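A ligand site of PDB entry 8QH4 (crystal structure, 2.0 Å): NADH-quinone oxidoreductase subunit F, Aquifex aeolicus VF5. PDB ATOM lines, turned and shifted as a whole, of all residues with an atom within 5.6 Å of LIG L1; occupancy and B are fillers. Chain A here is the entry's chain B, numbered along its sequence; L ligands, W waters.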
ATOM      1  N   GLY A  67      18.633  24.204 -11.668  1.00  0.00           N
ATOM      2  CA  GLY A  67      17.441  24.273 -12.505  1.00  0.00           C
ATOM      3  C   GLY A  67      16.251  24.904 -11.779  1.00  0.00           C
ATOM      4  O   GLY A  67      15.172  25.050 -12.359  1.00  0.00           O
ATOM      5  N   GLY A  68      16.437  25.215 -10.482  1.00  0.00           N
ATOM      6  CA  GLY A  68      15.420  25.931  -9.736  1.00  0.00           C
ATOM      7  C   GLY A  68      15.197  25.394  -8.316  1.00  0.00           C
ATOM      8  O   GLY A  68      14.882  26.192  -7.432  1.00  0.00           O
ATOM      9  N   ALA A  69      15.363  24.084  -8.088  1.00  0.00           N
ATOM     10  CA  ALA A  69      14.974  23.462  -6.823  1.00  0.00           C
ATOM     11  C   ALA A  69      16.156  23.302  -5.866  1.00  0.00           C
ATOM     12  O   ALA A  69      15.937  23.087  -4.672  1.00  0.00           O
ATOM     13  CB  ALA A  69      14.301  22.125  -7.082  1.00  0.00           C
ATOM     14  N   PHE A  71      18.402  20.864  -5.402  1.00  0.00           N
ATOM     15  CA  PHE A  71      18.652  19.558  -4.813  1.00  0.00           C
ATOM     16  C   PHE A  71      20.155  19.246  -4.916  1.00  0.00           C
ATOM     17  O   PHE A  71      20.804  19.536  -5.933  1.00  0.00           O
ATOM     18  CB  PHE A  71      17.753  18.486  -5.440  1.00  0.00           C
ATOM     19  CG  PHE A  71      17.752  17.160  -4.714  1.00  0.00           C
ATOM     20  CD1 PHE A  71      18.696  16.195  -5.007  1.00  0.00           C
ATOM     21  CD2 PHE A  71      16.849  16.899  -3.690  1.00  0.00           C
ATOM     22  CE1 PHE A  71      18.724  14.981  -4.334  1.00  0.00           C
ATOM     23  CE2 PHE A  71      16.878  15.685  -3.007  1.00  0.00           C
ATOM     24  CZ  PHE A  71      17.817  14.721  -3.329  1.00  0.00           C
ATOM     25  N   LYS A  76      21.728  13.140  -5.478  1.00  0.00           N
ATOM     26  CA  LYS A  76      20.840  12.671  -6.538  1.00  0.00           C
ATOM     27  C   LYS A  76      21.486  11.489  -7.250  1.00  0.00           C
ATOM     28  O   LYS A  76      20.840  10.474  -7.495  1.00  0.00           O
ATOM     29  CB  LYS A  76      20.509  13.783  -7.524  1.00  0.00           C
ATOM     30  CG  LYS A  76      19.363  13.448  -8.472  1.00  0.00           C
ATOM     31  CD  LYS A  76      19.178  14.426  -9.611  1.00  0.00           C
ATOM     32  CE  LYS A  76      18.823  15.827  -9.160  1.00  0.00           C
ATOM     33  NZ  LYS A  76      18.406  16.667 -10.311  1.00  0.00           N
ATOM     34  N   PHE A  79      21.396   8.258  -5.187  1.00  0.00           N
ATOM     35  CA  PHE A  79      20.077   7.636  -5.236  1.00  0.00           C
ATOM     36  C   PHE A  79      19.948   6.793  -6.507  1.00  0.00           C
ATOM     37  O   PHE A  79      19.478   5.650  -6.442  1.00  0.00           O
ATOM     38  CB  PHE A  79      18.950   8.668  -5.132  1.00  0.00           C
ATOM     39  CG  PHE A  79      18.616   9.121  -3.725  1.00  0.00           C
ATOM     40  CD1 PHE A  79      18.052   8.242  -2.821  1.00  0.00           C
ATOM     41  CD2 PHE A  79      18.843  10.430  -3.323  1.00  0.00           C
ATOM     42  CE1 PHE A  79      17.727   8.654  -1.529  1.00  0.00           C
ATOM     43  CE2 PHE A  79      18.527  10.844  -2.033  1.00  0.00           C
ATOM     44  CZ  PHE A  79      17.973   9.957  -1.141  1.00  0.00           C
ATOM     45  N   GLU A  97      11.517  29.513 -18.631  1.00  0.00           N
ATOM     46  CA  GLU A  97      10.910  30.390 -17.660  1.00  0.00           C
ATOM     47  C   GLU A  97      11.187  31.859 -18.006  1.00  0.00           C
ATOM     48  O   GLU A  97      12.326  32.202 -18.308  1.00  0.00           O
ATOM     49  CB  GLU A  97      11.424  30.136 -16.246  1.00  0.00           C
ATOM     50  CG  GLU A  97      10.512  30.784 -15.226  1.00  0.00           C
ATOM     51  CD  GLU A  97      10.828  30.518 -13.776  1.00  0.00           C
ATOM     52  OE1 GLU A  97      11.653  29.605 -13.506  1.00  0.00           O
ATOM     53  OE2 GLU A  97      10.271  31.250 -12.930  1.00  0.00           O
ATOM     54  N   TYR A 180       6.490  24.794 -22.108  1.00  0.00           N
ATOM     55  CA  TYR A 180       7.291  25.094 -20.925  1.00  0.00           C
ATOM     56  C   TYR A 180       7.332  23.924 -19.948  1.00  0.00           C
ATOM     57  O   TYR A 180       8.341  23.706 -19.265  1.00  0.00           O
ATOM     58  CB  TYR A 180       6.737  26.335 -20.208  1.00  0.00           C
ATOM     59  CG  TYR A 180       7.216  26.534 -18.795  1.00  0.00           C
ATOM     60  CD1 TYR A 180       8.537  26.846 -18.522  1.00  0.00           C
ATOM     61  CD2 TYR A 180       6.345  26.451 -17.722  1.00  0.00           C
ATOM     62  CE1 TYR A 180       8.987  27.037 -17.226  1.00  0.00           C
ATOM     63  CE2 TYR A 180       6.778  26.628 -16.423  1.00  0.00           C
ATOM     64  CZ  TYR A 180       8.109  26.932 -16.162  1.00  0.00           C
ATOM     65  OH  TYR A 180       8.557  27.123 -14.876  1.00  0.00           O
ATOM     66  N   GLU A 184       9.836  20.411 -16.774  1.00  0.00           N
ATOM     67  CA  GLU A 184       9.588  19.589 -15.602  1.00  0.00           C
ATOM     68  C   GLU A 184      10.098  18.191 -15.938  1.00  0.00           C
ATOM     69  O   GLU A 184       9.792  17.666 -17.005  1.00  0.00           O
ATOM     70  CB  GLU A 184       8.094  19.589 -15.245  1.00  0.00           C
ATOM     71  CG  GLU A 184       7.787  19.078 -13.860  1.00  0.00           C
ATOM     72  CD  GLU A 184       7.731  17.562 -13.668  1.00  0.00           C
ATOM     73  OE1 GLU A 184       7.752  16.833 -14.659  1.00  0.00           O
ATOM     74  OE2 GLU A 184       7.678  17.137 -12.500  1.00  0.00           O
ATOM     75  N   GLU A 185      10.882  17.596 -15.052  1.00  0.00           N
ATOM     76  CA  GLU A 185      11.753  16.491 -15.457  1.00  0.00           C
ATOM     77  C   GLU A 185      10.934  15.281 -15.919  1.00  0.00           C
ATOM     78  O   GLU A 185      11.375  14.560 -16.815  1.00  0.00           O
ATOM     79  CB  GLU A 185      12.701  16.118 -14.320  1.00  0.00           C
ATOM     80  CG  GLU A 185      11.979  15.825 -13.015  1.00  0.00           C
ATOM     81  CD  GLU A 185      12.878  15.400 -11.860  1.00  0.00           C
ATOM     82  OE1 GLU A 185      14.131  15.420 -12.029  1.00  0.00           O
ATOM     83  OE2 GLU A 185      12.322  15.045 -10.811  1.00  0.00           O
ATOM     84  N   LYS A 202       5.106  12.052  -8.709  1.00  0.00           N
ATOM     85  CA  LYS A 202       6.348  11.797  -7.989  1.00  0.00           C
ATOM     86  C   LYS A 202       6.050  11.721  -6.492  1.00  0.00           C
ATOM     87  O   LYS A 202       5.278  12.543  -5.991  1.00  0.00           O
ATOM     88  CB  LYS A 202       7.374  12.930  -8.208  1.00  0.00           C
ATOM     89  CG  LYS A 202       7.863  13.143  -9.635  1.00  0.00           C
ATOM     90  CD  LYS A 202       9.106  14.036  -9.738  1.00  0.00           C
ATOM     91  CE  LYS A 202       8.862  15.511  -9.448  1.00  0.00           C
ATOM     92  NZ  LYS A 202      10.005  16.374  -9.858  1.00  0.00           N
ATOM     93  N   TYR A 205      10.694   9.137  -8.072  1.00  0.00           N
ATOM     94  CA  TYR A 205      11.562  10.103  -8.734  1.00  0.00           C
ATOM     95  C   TYR A 205      12.246   9.419  -9.916  1.00  0.00           C
ATOM     96  O   TYR A 205      12.374   8.191  -9.974  1.00  0.00           O
ATOM     97  CB  TYR A 205      12.508  10.718  -7.701  1.00  0.00           C
ATOM     98  CG  TYR A 205      11.820  11.639  -6.724  1.00  0.00           C
ATOM     99  CD1 TYR A 205      11.539  12.954  -7.063  1.00  0.00           C
ATOM    100  CD2 TYR A 205      11.400  11.187  -5.490  1.00  0.00           C
ATOM    101  CE1 TYR A 205      10.880  13.806  -6.185  1.00  0.00           C
ATOM    102  CE2 TYR A 205      10.738  12.017  -4.592  1.00  0.00           C
ATOM    103  CZ  TYR A 205      10.487  13.328  -4.946  1.00  0.00           C
ATOM    104  OH  TYR A 205       9.828  14.170  -4.079  1.00  0.00           O
ATOM    105  N   PRO A 206      12.675  10.206 -10.930  1.00  0.00           N
ATOM    106  CA  PRO A 206      13.374   9.657 -12.091  1.00  0.00           C
ATOM    107  C   PRO A 206      14.538   8.736 -11.742  1.00  0.00           C
ATOM    108  O   PRO A 206      14.765   7.765 -12.452  1.00  0.00           O
ATOM    109  CB  PRO A 206      13.843  10.925 -12.824  1.00  0.00           C
ATOM    110  CG  PRO A 206      12.772  11.934 -12.497  1.00  0.00           C
ATOM    111  CD  PRO A 206      12.456  11.662 -11.042  1.00  0.00           C
ATOM    112  N   VAL A 207      15.222   9.005 -10.609  1.00  0.00           N
ATOM    113  CA  VAL A 207      16.398   8.238 -10.237  1.00  0.00           C
ATOM    114  C   VAL A 207      16.024   6.799  -9.873  1.00  0.00           C
ATOM    115  O   VAL A 207      16.876   5.910  -9.892  1.00  0.00           O
ATOM    116  CB  VAL A 207      17.230   8.939  -9.150  1.00  0.00           C
ATOM    117  CG1 VAL A 207      17.880  10.210  -9.682  1.00  0.00           C
ATOM    118  CG2 VAL A 207      16.421   9.223  -7.874  1.00  0.00           C
ATOM    119  N   VAL A 218      18.200  13.499 -14.115  1.00  0.00           N
ATOM    120  CA  VAL A 218      18.032  14.730 -14.854  1.00  0.00           C
ATOM    121  C   VAL A 218      18.776  15.836 -14.126  1.00  0.00           C
ATOM    122  O   VAL A 218      18.588  16.016 -12.926  1.00  0.00           O
ATOM    123  CB  VAL A 218      16.548  15.115 -15.027  1.00  0.00           C
ATOM    124  CG1 VAL A 218      16.420  16.390 -15.842  1.00  0.00           C
ATOM    125  CG2 VAL A 218      15.736  13.979 -15.651  1.00  0.00           C
ATOM    126  N   LEU A 297       8.338  33.170 -10.455  1.00  0.00           N
ATOM    127  CA  LEU A 297       8.244  32.416  -9.218  1.00  0.00           C
ATOM    128  C   LEU A 297       7.942  33.319  -8.018  1.00  0.00           C
ATOM    129  O   LEU A 297       6.982  33.067  -7.299  1.00  0.00           O
ATOM    130  CB  LEU A 297       9.556  31.646  -9.014  1.00  0.00           C
ATOM    131  CG  LEU A 297       9.645  30.775  -7.762  1.00  0.00           C
ATOM    132  CD1 LEU A 297       8.624  29.649  -7.799  1.00  0.00           C
ATOM    133  CD2 LEU A 297      11.051  30.192  -7.621  1.00  0.00           C
ATOM    134  N   GLY A 318      15.595  30.156  -6.405  1.00  0.00           N
ATOM    135  CA  GLY A 318      15.239  29.888  -7.791  1.00  0.00           C
ATOM    136  C   GLY A 318      16.452  29.557  -8.665  1.00  0.00           C
ATOM    137  O   GLY A 318      17.286  28.731  -8.303  1.00  0.00           O
ATOM    138  N   THR A 319      16.502  30.195  -9.826  1.00  0.00           N
ATOM    139  CA  THR A 319      17.615  30.033 -10.769  1.00  0.00           C
ATOM    140  C   THR A 319      18.513  31.278 -10.757  1.00  0.00           C
ATOM    141  O   THR A 319      19.428  31.364 -11.574  1.00  0.00           O
ATOM    142  CB  THR A 319      17.040  29.762 -12.165  1.00  0.00           C
ATOM    143  OG1 THR A 319      16.055  30.773 -12.393  1.00  0.00           O
ATOM    144  CG2 THR A 319      16.421  28.386 -12.283  1.00  0.00           C
ATOM    145  N   GLY A 394       5.043  20.980 -10.015  1.00  0.00           N
ATOM    146  CA  GLY A 394       5.391  22.247  -9.393  1.00  0.00           C
ATOM    147  C   GLY A 394       4.699  23.465 -10.004  1.00  0.00           C
ATOM    148  O   GLY A 394       4.593  24.505  -9.345  1.00  0.00           O
ATOM    149  N   LEU A 395       4.232  23.340 -11.254  1.00  0.00           N
ATOM    150  CA  LEU A 395       3.580  24.458 -11.937  1.00  0.00           C
ATOM    151  C   LEU A 395       2.295  24.865 -11.200  1.00  0.00           C
ATOM    152  O   LEU A 395       2.095  26.043 -10.907  1.00  0.00           O
ATOM    153  CB  LEU A 395       3.318  24.081 -13.394  1.00  0.00           C
ATOM    154  CG  LEU A 395       2.850  25.231 -14.283  1.00  0.00           C
ATOM    155  CD1 LEU A 395       3.222  24.992 -15.742  1.00  0.00           C
ATOM    156  CD2 LEU A 395       1.337  25.426 -14.151  1.00  0.00           C
ATOM    157  N   VAL A 398       2.836  26.733  -7.901  1.00  0.00           N
ATOM    158  CA  VAL A 398       3.396  28.071  -7.865  1.00  0.00           C
ATOM    159  C   VAL A 398       2.694  29.035  -8.838  1.00  0.00           C
ATOM    160  O   VAL A 398       3.061  30.205  -8.863  1.00  0.00           O
ATOM    161  CB  VAL A 398       4.925  28.072  -8.137  1.00  0.00           C
ATOM    162  CG1 VAL A 398       5.681  27.220  -7.141  1.00  0.00           C
ATOM    163  CG2 VAL A 398       5.261  27.660  -9.543  1.00  0.00           C
HETATM  164  P1  LIG L   1      11.762  18.978  -6.712  1.00  0.00           P
HETATM  165  O1  LIG L   1      12.127  19.612  -5.419  1.00  0.00           O
HETATM  166  O2  LIG L   1      10.600  18.061  -6.767  1.00  0.00           O
HETATM  167  O3  LIG L   1      13.039  18.135  -7.205  1.00  0.00           O
HETATM  168  C1  LIG L   1      14.319  18.732  -7.516  1.00  0.00           C
HETATM  169  C2  LIG L   1      15.222  17.652  -8.059  1.00  0.00           C
HETATM  170  O4  LIG L   1      15.613  16.781  -6.975  1.00  0.00           O
HETATM  171  C3  LIG L   1      14.606  16.738  -9.120  1.00  0.00           C
HETATM  172  O5  LIG L   1      15.605  16.241 -10.000  1.00  0.00           O
HETATM  173  C4  LIG L   1      14.037  15.586  -8.284  1.00  0.00           C
HETATM  174  O6  LIG L   1      13.946  14.347  -9.004  1.00  0.00           O
HETATM  175  C5  LIG L   1      15.107  15.476  -7.193  1.00  0.00           C
HETATM  176  N1  LIG L   1      14.589  14.972  -5.931  1.00  0.00           N
HETATM  177  C6  LIG L   1      13.818  15.645  -5.018  1.00  0.00           C
HETATM  178  N2  LIG L   1      13.473  14.934  -3.967  1.00  0.00           N
HETATM  179  C7  LIG L   1      14.070  13.700  -4.203  1.00  0.00           C
HETATM  180  C8  LIG L   1      14.095  12.502  -3.468  1.00  0.00           C
HETATM  181  N3  LIG L   1      13.449  12.315  -2.306  1.00  0.00           N
HETATM  182  N4  LIG L   1      14.776  11.457  -3.989  1.00  0.00           N
HETATM  183  C9  LIG L   1      15.405  11.611  -5.169  1.00  0.00           C
HETATM  184  N5  LIG L   1      15.448  12.693  -5.950  1.00  0.00           N
HETATM  185  C10 LIG L   1      14.767  13.706  -5.409  1.00  0.00           C
HETATM  186  O7  LIG L   1      11.578  20.156  -7.785  1.00  0.00           O
HETATM  187  P2  LIG L   1      10.949  20.268  -9.252  1.00  0.00           P
HETATM  188  O8  LIG L   1      11.742  19.426 -10.185  1.00  0.00           O
HETATM  189  O9  LIG L   1       9.473  20.096  -9.178  1.00  0.00           O
HETATM  190  O10 LIG L   1      11.309  21.766  -9.623  1.00  0.00           O
HETATM  191  C11 LIG L   1      10.609  22.872  -9.015  1.00  0.00           C
HETATM  192  C12 LIG L   1      11.316  24.155  -9.385  1.00  0.00           C
HETATM  193  O11 LIG L   1      11.014  24.520 -10.753  1.00  0.00           O
HETATM  194  C13 LIG L   1      10.924  25.348  -8.516  1.00  0.00           C
HETATM  195  O12 LIG L   1      11.862  25.489  -7.454  1.00  0.00           O
HETATM  196  C14 LIG L   1      10.985  26.509  -9.512  1.00  0.00           C
HETATM  197  O13 LIG L   1      12.304  27.030  -9.639  1.00  0.00           O
HETATM  198  C15 LIG L   1      10.482  25.815 -10.781  1.00  0.00           C
HETATM  199  N6  LIG L   1       8.976  25.727 -10.832  1.00  0.00           N
HETATM  200  C1  LG2 L   2      11.200  22.717 -14.032  1.00  0.00           C
HETATM  201  N1  LG2 L   2      12.598  22.441 -13.921  1.00  0.00           N
HETATM  202  C2  LG2 L   2      13.447  22.864 -14.940  1.00  0.00           C
HETATM  203  N2  LG2 L   2      14.768  22.506 -14.889  1.00  0.00           N
HETATM  204  C3  LG2 L   2      15.676  22.835 -15.861  1.00  0.00           C
HETATM  205  O1  LG2 L   2      16.846  22.466 -15.802  1.00  0.00           O
HETATM  206  N3  LG2 L   2      15.179  23.550 -16.919  1.00  0.00           N
HETATM  207  C4  LG2 L   2      13.872  23.971 -17.104  1.00  0.00           C
HETATM  208  O2  LG2 L   2      13.590  24.654 -18.091  1.00  0.00           O
HETATM  209  C5  LG2 L   2      12.976  23.557 -16.045  1.00  0.00           C
HETATM  210  N4  LG2 L   2      11.646  23.815 -16.148  1.00  0.00           N
HETATM  211  C6  LG2 L   2      10.740  23.374 -15.180  1.00  0.00           C
HETATM  212  C7  LG2 L   2       9.380  23.629 -15.339  1.00  0.00           C
HETATM  213  C8  LG2 L   2       8.465  23.237 -14.367  1.00  0.00           C
HETATM  214  C9  LG2 L   2       7.010  23.586 -14.537  1.00  0.00           C
HETATM  215  C10 LG2 L   2       8.926  22.580 -13.209  1.00  0.00           C
HETATM  216  C11 LG2 L   2       7.969  22.211 -12.097  1.00  0.00           C
HETATM  217  C12 LG2 L   2      10.279  22.312 -13.049  1.00  0.00           C
HETATM  218  C13 LG2 L   2      13.130  21.668 -12.800  1.00  0.00           C
HETATM  219  C14 LG2 L   2      13.274  20.189 -13.193  1.00  0.00           C
HETATM  220  O3  LG2 L   2      12.023  19.532 -12.960  1.00  0.00           O
HETATM  221  C15 LG2 L   2      14.366  19.528 -12.345  1.00  0.00           C
HETATM  222  O4  LG2 L   2      14.262  19.939 -10.981  1.00  0.00           O
HETATM  223  C16 LG2 L   2      15.809  19.858 -12.764  1.00  0.00           C
HETATM  224  O5  LG2 L   2      15.995  19.753 -14.175  1.00  0.00           O
HETATM  225  C17 LG2 L   2      16.803  18.970 -12.047  1.00  0.00           C
HETATM  226  O6  LG2 L   2      18.132  19.434 -12.360  1.00  0.00           O
HETATM  227  P1  LG2 L   2      19.035  20.187 -11.224  1.00  0.00           P
HETATM  228  O7  LG2 L   2      18.975  19.308  -9.997  1.00  0.00           O
HETATM  229  O8  LG2 L   2      20.420  20.223 -11.855  1.00  0.00           O
HETATM  230  O9  LG2 L   2      18.434  21.565 -11.014  1.00  0.00           O
HETATM  231  O   HOH W   1      12.022  16.646  -2.126  1.00  0.00           O
HETATM  232  O   HOH W   2      11.710  14.375  -1.368  1.00  0.00           O
HETATM  233  O   HOH W   3      15.519  12.403  -9.104  1.00  0.00           O
HETATM  234  O   HOH W   4       7.925  21.318  -7.017  1.00  0.00           O
HETATM  235  O   HOH W   5       7.527  24.548  -8.563  1.00  0.00           O
HETATM  236  O   HOH W   6       7.207  27.162 -12.622  1.00  0.00           O
HETATM  237  O   HOH W   7       7.279  19.214 -10.314  1.00  0.00           O
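An oxygen (O8) of LIG L1 is in hydrogen-bond range of an oxygen (O4) of LG2 L2 (2.7 Å).
Merely in contact with LIG L1: Ala 69, Phe 71, Tyr 205, Pro 206, Val 207 and Leu 297. Within 4 Å of LIG L1: Gly 68, Ala 69, Phe 71, Lys 76, Glu 185, Lys 202, Tyr 205, Pro 206, Val 207 and Leu 297. The nearest printed residue that does not touch LIG L1 is Phe 79 (4.1 Å).
Water W7 lies within hydrogen-bond range of O9 of LIG L1 (2.6 Å), N of Gly 394 (2.9 Å) and OE2 of Glu 184 (3.0 Å). Water W2 lies within hydrogen-bond range of N3 of LIG L1 (2.9 Å) and OH of Tyr 205 (3.3 Å). Water W6 bridges OH of Tyr 180 (2.6 Å) and N6 of LIG L1 (2.9 Å). Water W5 lies within hydrogen-bond range of a nitrogen (N6) of LIG L1 (2.9 Å) and the backbone carbonyl oxygen of Gly 394 (3.0 Å).
OE2 of Glu 185 lies within salt-bridge range of NZ of Lys 202, 2.8 Å away. The side-chain amino group (NZ) of Lys 76 sits at hydrogen-bond distance from the backbone carbonyl oxygen (O) of Val 218 (2.7 Å). NZ of Lys 202 lies within salt-bridge range of OE2 of Glu 184.
An oxygen (O6) of LIG L1 sits at hydrogen-bond distance from the side-chain carboxylate (OE2) of Glu 185 (2.5 Å). The side-chain amino group (NZ) of Lys 76 is in hydrogen-bond range of an oxygen (O5) of LIG L1, at 2.9 Å. O12 of LIG L1 sits at hydrogen-bond distance from O of Gly 68 (3.1 Å). The side-chain amino group (NZ) of Lys 202 lies within salt-bridge range of an oxygen (O8) of LIG L1 (3.5 Å). N of Glu 185 lies within hydrogen-bond range of O3 of LG2 L2, at 3.1 Å. O7 of LG2 L2 lies within salt-bridge range of NZ of Lys 76, at 2.7 Å. N of Gly 67 lies within hydrogen-bond range of O9 of LG2 L2, at 2.7 Å.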
